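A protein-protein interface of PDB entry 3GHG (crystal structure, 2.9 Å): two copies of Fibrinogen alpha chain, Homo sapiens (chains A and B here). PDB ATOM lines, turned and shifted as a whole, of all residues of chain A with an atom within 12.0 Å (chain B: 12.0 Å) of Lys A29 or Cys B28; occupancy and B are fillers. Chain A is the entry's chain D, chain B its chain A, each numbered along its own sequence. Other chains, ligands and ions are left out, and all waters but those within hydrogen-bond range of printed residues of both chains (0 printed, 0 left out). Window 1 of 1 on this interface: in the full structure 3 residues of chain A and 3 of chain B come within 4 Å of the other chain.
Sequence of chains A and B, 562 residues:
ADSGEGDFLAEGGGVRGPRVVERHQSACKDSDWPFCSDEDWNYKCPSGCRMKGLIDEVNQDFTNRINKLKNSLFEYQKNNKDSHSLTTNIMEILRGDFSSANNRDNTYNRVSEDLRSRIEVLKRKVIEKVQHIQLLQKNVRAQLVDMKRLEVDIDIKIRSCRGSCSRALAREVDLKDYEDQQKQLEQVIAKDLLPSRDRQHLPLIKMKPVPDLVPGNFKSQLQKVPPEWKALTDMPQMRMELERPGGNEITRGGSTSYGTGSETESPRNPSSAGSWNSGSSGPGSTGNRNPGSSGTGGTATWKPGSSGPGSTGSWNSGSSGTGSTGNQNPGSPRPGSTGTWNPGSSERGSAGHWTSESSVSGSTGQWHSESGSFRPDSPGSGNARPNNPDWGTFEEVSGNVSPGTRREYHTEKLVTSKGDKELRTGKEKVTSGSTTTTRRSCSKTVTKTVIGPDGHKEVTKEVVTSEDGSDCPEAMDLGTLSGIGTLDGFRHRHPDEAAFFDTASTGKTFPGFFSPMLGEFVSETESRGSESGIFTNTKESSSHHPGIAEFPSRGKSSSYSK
The side-chain sulfur of Cys B28 forms a disulfide with the side-chain sulfur of Cys A28 (2.0 Å).
N of Ala B27 sits at hydrogen-bond distance from OD2 of Asp B30.
O of Cys A28 lies within hydrogen-bond range of NE1 of Trp A33 (3.1 Å).
OG of Ser A31 is in hydrogen-bond range of O of Lys A29 (3.1 Å).
The backbone carbonyl oxygen (O) of Lys B29 is in hydrogen-bond range of the side-chain hydroxyl (OG) of Ser B31 (3.0 Å).
Lys B29 touches Ala A27.
Ala B27 touches Lys A29 (CA to CD, 3.9 Å).
CB of Cys B28 touches N of Lys A29 (3.3 Å).
Ala A27 touches just one residue of chain B: Lys B29 (3.7 Å).
Lys A29 touches just these residues of chain B: Ala B27 (3.9 Å) and Cys B28 (3.3 Å).
No residue of chain B comes within 4 Å of Asp A30.
Printed residues of chain A within 4 Å of Cys B28: Cys A28 (2.0 Å) and Lys A29 (3.3 Å).
Of the printed residues of chain A, Lys B29 touches Ala A27.
The nearest residue of chain B that does not touch Lys A29 is Lys B29 (5.6 Å).
The nearest printed residue of chain A that does not touch Lys B29 is Cys A28 (5.5 Å).
Of the 12 printed residues of chain A, 3 touch a printed residue of chain B.
Printed residues of chain A that touch a printed residue of chain B: Ala A27, Cys A28 and Lys A29.
Ala A27 touches Lys B29, and with the chains exchanged Lys A29 touches Ala B27.
Cys B28 touches its own counterpart, Cys A28.
Lys A29 touches Cys B28, but with the chains exchanged Cys A28 does not touch Lys B29 (5.5 Å).
Positions printed for both chains: 27, 28, 29, 30, 31, 32, 33, 47, 49 and 50.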
ATOM      1  N   ALA A  27      33.666  -3.478 -26.287  1.00  0.00           N
ATOM      2  CA  ALA A  27      32.482  -4.319 -25.953  1.00  0.00           C
ATOM      3  C   ALA A  27      31.177  -3.672 -26.423  1.00  0.00           C
ATOM      4  O   ALA A  27      31.077  -2.447 -26.525  1.00  0.00           O
ATOM      5  CB  ALA A  27      32.431  -4.579 -24.450  1.00  0.00           C
ATOM      6  N   CYS A  28      30.183  -4.513 -26.702  1.00  0.00           N
ATOM      7  CA  CYS A  28      28.823  -4.065 -27.017  1.00  0.00           C
ATOM      8  C   CYS A  28      28.029  -3.776 -25.736  1.00  0.00           C
ATOM      9  O   CYS A  28      26.888  -3.307 -25.796  1.00  0.00           O
ATOM     10  CB  CYS A  28      28.097  -5.133 -27.843  1.00  0.00           C
ATOM     11  SG  CYS A  28      27.432  -6.520 -26.868  1.00  0.00           S
ATOM     12  N   LYS A  29      28.642  -4.076 -24.588  1.00  0.00           N
ATOM     13  CA  LYS A  29      28.052  -3.846 -23.267  1.00  0.00           C
ATOM     14  C   LYS A  29      27.859  -2.355 -23.024  1.00  0.00           C
ATOM     15  O   LYS A  29      26.829  -1.938 -22.480  1.00  0.00           O
ATOM     16  CB  LYS A  29      28.964  -4.422 -22.174  1.00  0.00           C
ATOM     17  CG  LYS A  29      28.304  -4.600 -20.808  1.00  0.00           C
ATOM     18  CD  LYS A  29      27.434  -5.848 -20.763  1.00  0.00           C
ATOM     19  CE  LYS A  29      26.620  -5.915 -19.482  1.00  0.00           C
ATOM     20  NZ  LYS A  29      25.559  -4.871 -19.446  1.00  0.00           N
ATOM     21  N   ASP A  30      28.868  -1.570 -23.413  1.00  0.00           N
ATOM     22  CA  ASP A  30      28.799  -0.108 -23.373  1.00  0.00           C
ATOM     23  C   ASP A  30      27.486   0.323 -24.026  1.00  0.00           C
ATOM     24  O   ASP A  30      27.415   0.534 -25.241  1.00  0.00           O
ATOM     25  CB  ASP A  30      30.017   0.512 -24.091  1.00  0.00           C
ATOM     26  CG  ASP A  30      30.279   1.964 -23.686  1.00  0.00           C
ATOM     27  OD1 ASP A  30      31.397   2.457 -23.951  1.00  0.00           O
ATOM     28  OD2 ASP A  30      29.385   2.617 -23.106  1.00  0.00           O
ATOM     29  N   SER A  31      26.442   0.421 -23.206  1.00  0.00           N
ATOM     30  CA  SER A  31      25.096   0.670 -23.702  1.00  0.00           C
ATOM     31  C   SER A  31      25.010   2.041 -24.364  1.00  0.00           C
ATOM     32  O   SER A  31      24.535   3.010 -23.769  1.00  0.00           O
ATOM     33  CB  SER A  31      24.064   0.536 -22.579  1.00  0.00           C
ATOM     34  OG  SER A  31      23.969  -0.809 -22.139  1.00  0.00           O
ATOM     35  N   ASP A  32      25.491   2.100 -25.605  1.00  0.00           N
ATOM     36  CA  ASP A  32      25.354   3.284 -26.453  1.00  0.00           C
ATOM     37  C   ASP A  32      23.954   3.348 -27.055  1.00  0.00           C
ATOM     38  O   ASP A  32      23.588   4.345 -27.677  1.00  0.00           O
ATOM     39  CB  ASP A  32      26.362   3.243 -27.608  1.00  0.00           C
ATOM     40  CG  ASP A  32      27.798   3.130 -27.137  1.00  0.00           C
ATOM     41  OD1 ASP A  32      28.139   3.732 -26.098  1.00  0.00           O
ATOM     42  OD2 ASP A  32      28.589   2.443 -27.820  1.00  0.00           O
ATOM     43  N   TRP A  33      23.177   2.284 -26.859  1.00  0.00           N
ATOM     44  CA  TRP A  33      21.946   2.073 -27.611  1.00  0.00           C
ATOM     45  C   TRP A  33      20.794   2.885 -26.992  1.00  0.00           C
ATOM     46  O   TRP A  33      20.759   3.081 -25.774  1.00  0.00           O
ATOM     47  CB  TRP A  33      21.589   0.569 -27.672  1.00  0.00           C
ATOM     48  CG  TRP A  33      22.779  -0.407 -27.693  1.00  0.00           C
ATOM     49  CD1 TRP A  33      23.348  -1.023 -26.609  1.00  0.00           C
ATOM     50  CD2 TRP A  33      23.509  -0.878 -28.843  1.00  0.00           C
ATOM     51  NE1 TRP A  33      24.386  -1.834 -27.009  1.00  0.00           N
ATOM     52  CE2 TRP A  33      24.506  -1.764 -28.372  1.00  0.00           C
ATOM     53  CE3 TRP A  33      23.421  -0.631 -30.221  1.00  0.00           C
ATOM     54  CZ2 TRP A  33      25.407  -2.406 -29.229  1.00  0.00           C
ATOM     55  CZ3 TRP A  33      24.321  -1.270 -31.072  1.00  0.00           C
ATOM     56  CH2 TRP A  33      25.298  -2.147 -30.569  1.00  0.00           C
ATOM     57  N   PRO A  34      19.859   3.378 -27.834  1.00  0.00           N
ATOM     58  CA  PRO A  34      18.630   4.028 -27.363  1.00  0.00           C
ATOM     59  C   PRO A  34      17.739   3.097 -26.536  1.00  0.00           C
ATOM     60  O   PRO A  34      18.195   2.046 -26.091  1.00  0.00           O
ATOM     61  CB  PRO A  34      17.919   4.419 -28.664  1.00  0.00           C
ATOM     62  CG  PRO A  34      18.983   4.517 -29.671  1.00  0.00           C
ATOM     63  CD  PRO A  34      19.998   3.490 -29.299  1.00  0.00           C
ATOM     64  N   PHE A  35      16.479   3.483 -26.337  1.00  0.00           N
ATOM     65  CA  PHE A  35      15.534   2.669 -25.568  1.00  0.00           C
ATOM     66  C   PHE A  35      14.395   2.151 -26.442  1.00  0.00           C
ATOM     67  O   PHE A  35      13.849   2.880 -27.270  1.00  0.00           O
ATOM     68  CB  PHE A  35      15.006   3.453 -24.363  1.00  0.00           C
ATOM     69  CG  PHE A  35      15.995   3.549 -23.229  1.00  0.00           C
ATOM     70  CD1 PHE A  35      15.822   2.803 -22.064  1.00  0.00           C
ATOM     71  CD2 PHE A  35      17.118   4.365 -23.339  1.00  0.00           C
ATOM     72  CE1 PHE A  35      16.741   2.883 -21.021  1.00  0.00           C
ATOM     73  CE2 PHE A  35      18.042   4.449 -22.303  1.00  0.00           C
ATOM     74  CZ  PHE A  35      17.854   3.708 -21.142  1.00  0.00           C
ATOM     75  N   SER A  47      18.820 -11.803 -28.725  1.00  0.00           N
ATOM     76  CA  SER A  47      19.762 -12.835 -29.204  1.00  0.00           C
ATOM     77  C   SER A  47      19.281 -14.249 -28.888  1.00  0.00           C
ATOM     78  O   SER A  47      18.699 -14.493 -27.832  1.00  0.00           O
ATOM     79  CB  SER A  47      21.164 -12.652 -28.600  1.00  0.00           C
ATOM     80  OG  SER A  47      21.501 -13.723 -27.721  1.00  0.00           O
ATOM     81  N   CYS A  49      21.034 -16.780 -28.103  1.00  0.00           N
ATOM     82  CA  CYS A  49      21.792 -17.345 -26.999  1.00  0.00           C
ATOM     83  C   CYS A  49      21.119 -16.986 -25.694  1.00  0.00           C
ATOM     84  O   CYS A  49      20.798 -17.850 -24.877  1.00  0.00           O
ATOM     85  CB  CYS A  49      23.214 -16.789 -26.981  1.00  0.00           C
ATOM     86  SG  CYS A  49      24.146 -17.095 -28.470  1.00  0.00           S
ATOM     87  N   ARG A  50      20.906 -15.691 -25.513  1.00  0.00           N
ATOM     88  CA  ARG A  50      20.317 -15.171 -24.292  1.00  0.00           C
ATOM     89  C   ARG A  50      18.824 -15.471 -24.221  1.00  0.00           C
ATOM     90  O   ARG A  50      18.237 -15.429 -23.142  1.00  0.00           O
ATOM     91  CB  ARG A  50      20.556 -13.670 -24.204  1.00  0.00           C
ATOM     92  CG  ARG A  50      20.538 -13.105 -22.799  1.00  0.00           C
ATOM     93  CD  ARG A  50      20.718 -11.595 -22.842  1.00  0.00           C
ATOM     94  NE  ARG A  50      21.950 -11.167 -23.526  1.00  0.00           N
ATOM     95  CZ  ARG A  50      22.036 -10.723 -24.788  1.00  0.00           C
ATOM     96  NH1 ARG A  50      20.963 -10.631 -25.572  1.00  0.00           N
ATOM     97  NH2 ARG A  50      23.220 -10.367 -25.279  1.00  0.00           N
ATOM     98  N   ALA B  27      30.765  -9.101 -18.850  1.00  0.00           N
ATOM     99  CA  ALA B  27      30.508  -8.077 -19.903  1.00  0.00           C
ATOM    100  C   ALA B  27      30.086  -8.741 -21.216  1.00  0.00           C
ATOM    101  O   ALA B  27      29.822  -9.945 -21.255  1.00  0.00           O
ATOM    102  CB  ALA B  27      31.751  -7.216 -20.110  1.00  0.00           C
ATOM    103  N   CYS B  28      30.015  -7.940 -22.278  1.00  0.00           N
ATOM    104  CA  CYS B  28      29.773  -8.433 -23.644  1.00  0.00           C
ATOM    105  C   CYS B  28      31.029  -9.147 -24.173  1.00  0.00           C
ATOM    106  O   CYS B  28      30.933 -10.080 -24.976  1.00  0.00           O
ATOM    107  CB  CYS B  28      29.376  -7.260 -24.570  1.00  0.00           C
ATOM    108  SG  CYS B  28      29.062  -7.643 -26.347  1.00  0.00           S
ATOM    109  N   LYS B  29      32.196  -8.702 -23.700  1.00  0.00           N
ATOM    110  CA  LYS B  29      33.503  -9.262 -24.089  1.00  0.00           C
ATOM    111  C   LYS B  29      33.703 -10.746 -23.752  1.00  0.00           C
ATOM    112  O   LYS B  29      34.404 -11.451 -24.483  1.00  0.00           O
ATOM    113  CB  LYS B  29      34.632  -8.457 -23.426  1.00  0.00           C
ATOM    114  CG  LYS B  29      35.077  -7.223 -24.198  1.00  0.00           C
ATOM    115  CD  LYS B  29      36.279  -7.523 -25.085  1.00  0.00           C
ATOM    116  CE  LYS B  29      36.907  -6.253 -25.631  1.00  0.00           C
ATOM    117  NZ  LYS B  29      38.288  -6.507 -26.123  1.00  0.00           N
ATOM    118  N   ASP B  30      33.099 -11.200 -22.651  1.00  0.00           N
ATOM    119  CA  ASP B  30      33.343 -12.541 -22.083  1.00  0.00           C
ATOM    120  C   ASP B  30      33.512 -13.658 -23.124  1.00  0.00           C
ATOM    121  O   ASP B  30      32.535 -14.307 -23.516  1.00  0.00           O
ATOM    122  CB  ASP B  30      32.219 -12.915 -21.101  1.00  0.00           C
ATOM    123  CG  ASP B  30      32.270 -12.107 -19.812  1.00  0.00           C
ATOM    124  OD1 ASP B  30      32.126 -12.710 -18.728  1.00  0.00           O
ATOM    125  OD2 ASP B  30      32.459 -10.873 -19.878  1.00  0.00           O
ATOM    126  N   SER B  31      34.758 -13.886 -23.547  1.00  0.00           N
ATOM    127  CA  SER B  31      35.088 -14.923 -24.533  1.00  0.00           C
ATOM    128  C   SER B  31      35.208 -16.292 -23.865  1.00  0.00           C
ATOM    129  O   SER B  31      36.223 -16.981 -24.008  1.00  0.00           O
ATOM    130  CB  SER B  31      36.393 -14.581 -25.264  1.00  0.00           C
ATOM    131  OG  SER B  31      36.311 -13.316 -25.897  1.00  0.00           O
ATOM    132  N   ASP B  32      34.152 -16.685 -23.152  1.00  0.00           N
ATOM    133  CA  ASP B  32      34.088 -17.978 -22.476  1.00  0.00           C
ATOM    134  C   ASP B  32      33.409 -18.991 -23.394  1.00  0.00           C
ATOM    135  O   ASP B  32      32.678 -19.865 -22.930  1.00  0.00           O
ATOM    136  CB  ASP B  32      33.295 -17.861 -21.168  1.00  0.00           C
ATOM    137  CG  ASP B  32      33.791 -16.737 -20.273  1.00  0.00           C
ATOM    138  OD1 ASP B  32      35.012 -16.475 -20.259  1.00  0.00           O
ATOM    139  OD2 ASP B  32      32.958 -16.119 -19.576  1.00  0.00           O
ATOM    140  N   TRP B  33      33.660 -18.871 -24.696  1.00  0.00           N
ATOM    141  CA  TRP B  33      32.969 -19.668 -25.700  1.00  0.00           C
ATOM    142  C   TRP B  33      33.985 -20.430 -26.552  1.00  0.00           C
ATOM    143  O   TRP B  33      35.019 -19.867 -26.932  1.00  0.00           O
ATOM    144  CB  TRP B  33      32.112 -18.764 -26.583  1.00  0.00           C
ATOM    145  CG  TRP B  33      31.230 -17.823 -25.813  1.00  0.00           C
ATOM    146  CD1 TRP B  33      31.506 -16.526 -25.487  1.00  0.00           C
ATOM    147  CD2 TRP B  33      29.931 -18.105 -25.277  1.00  0.00           C
ATOM    148  NE1 TRP B  33      30.459 -15.982 -24.779  1.00  0.00           N
ATOM    149  CE2 TRP B  33      29.480 -16.929 -24.636  1.00  0.00           C
ATOM    150  CE3 TRP B  33      29.104 -19.236 -25.275  1.00  0.00           C
ATOM    151  CZ2 TRP B  33      28.237 -16.852 -24.000  1.00  0.00           C
ATOM    152  CZ3 TRP B  33      27.869 -19.160 -24.641  1.00  0.00           C
ATOM    153  CH2 TRP B  33      27.449 -17.975 -24.013  1.00  0.00           C
ATOM    154  N   PRO B  46      24.767 -15.189 -36.494  1.00  0.00           N
ATOM    155  CA  PRO B  46      25.335 -13.963 -35.931  1.00  0.00           C
ATOM    156  C   PRO B  46      24.297 -12.884 -35.664  1.00  0.00           C
ATOM    157  O   PRO B  46      23.404 -12.680 -36.484  1.00  0.00           O
ATOM    158  CB  PRO B  46      26.277 -13.496 -37.036  1.00  0.00           C
ATOM    159  CG  PRO B  46      25.577 -13.897 -38.297  1.00  0.00           C
ATOM    160  CD  PRO B  46      24.726 -15.114 -37.968  1.00  0.00           C
ATOM    161  N   SER B  47      24.438 -12.181 -34.542  1.00  0.00           N
ATOM    162  CA  SER B  47      23.451 -11.181 -34.129  1.00  0.00           C
ATOM    163  C   SER B  47      23.294 -10.096 -35.190  1.00  0.00           C
ATOM    164  O   SER B  47      24.278  -9.521 -35.650  1.00  0.00           O
ATOM    165  CB  SER B  47      23.833 -10.548 -32.780  1.00  0.00           C
ATOM    166  OG  SER B  47      24.918  -9.639 -32.907  1.00  0.00           O
ATOM    167  N   GLY B  48      22.046  -9.824 -35.563  1.00  0.00           N
ATOM    168  CA  GLY B  48      21.725  -8.806 -36.550  1.00  0.00           C
ATOM    169  C   GLY B  48      22.427  -7.469 -36.357  1.00  0.00           C
ATOM    170  O   GLY B  48      22.718  -6.781 -37.336  1.00  0.00           O
ATOM    171  N   CYS B  49      22.699  -7.100 -35.104  1.00  0.00           N
ATOM    172  CA  CYS B  49      23.382  -5.836 -34.779  1.00  0.00           C
ATOM    173  C   CYS B  49      24.708  -5.660 -35.510  1.00  0.00           C
ATOM    174  O   CYS B  49      24.964  -4.629 -36.145  1.00  0.00           O
ATOM    175  CB  CYS B  49      23.664  -5.749 -33.279  1.00  0.00           C
ATOM    176  SG  CYS B  49      22.217  -5.460 -32.272  1.00  0.00           S
ATOM    177  N   ARG B  50      25.562  -6.667 -35.382  1.00  0.00           N
ATOM    178  CA  ARG B  50      26.852  -6.661 -36.048  1.00  0.00           C
ATOM    179  C   ARG B  50      26.614  -6.797 -37.536  1.00  0.00           C
ATOM    180  O   ARG B  50      27.308  -6.179 -38.329  1.00  0.00           O
ATOM    181  CB  ARG B  50      27.722  -7.800 -35.534  1.00  0.00           C
ATOM    182  CG  ARG B  50      29.222  -7.569 -35.647  1.00  0.00           C
ATOM    183  CD  ARG B  50      30.000  -8.697 -34.969  1.00  0.00           C
ATOM    184  NE  ARG B  50      29.232  -9.375 -33.912  1.00  0.00           N
ATOM    185  CZ  ARG B  50      28.530 -10.508 -34.059  1.00  0.00           C
ATOM    186  NH1 ARG B  50      28.468 -11.145 -35.231  1.00  0.00           N
ATOM    187  NH2 ARG B  50      27.873 -11.015 -33.018  1.00  0.00           N
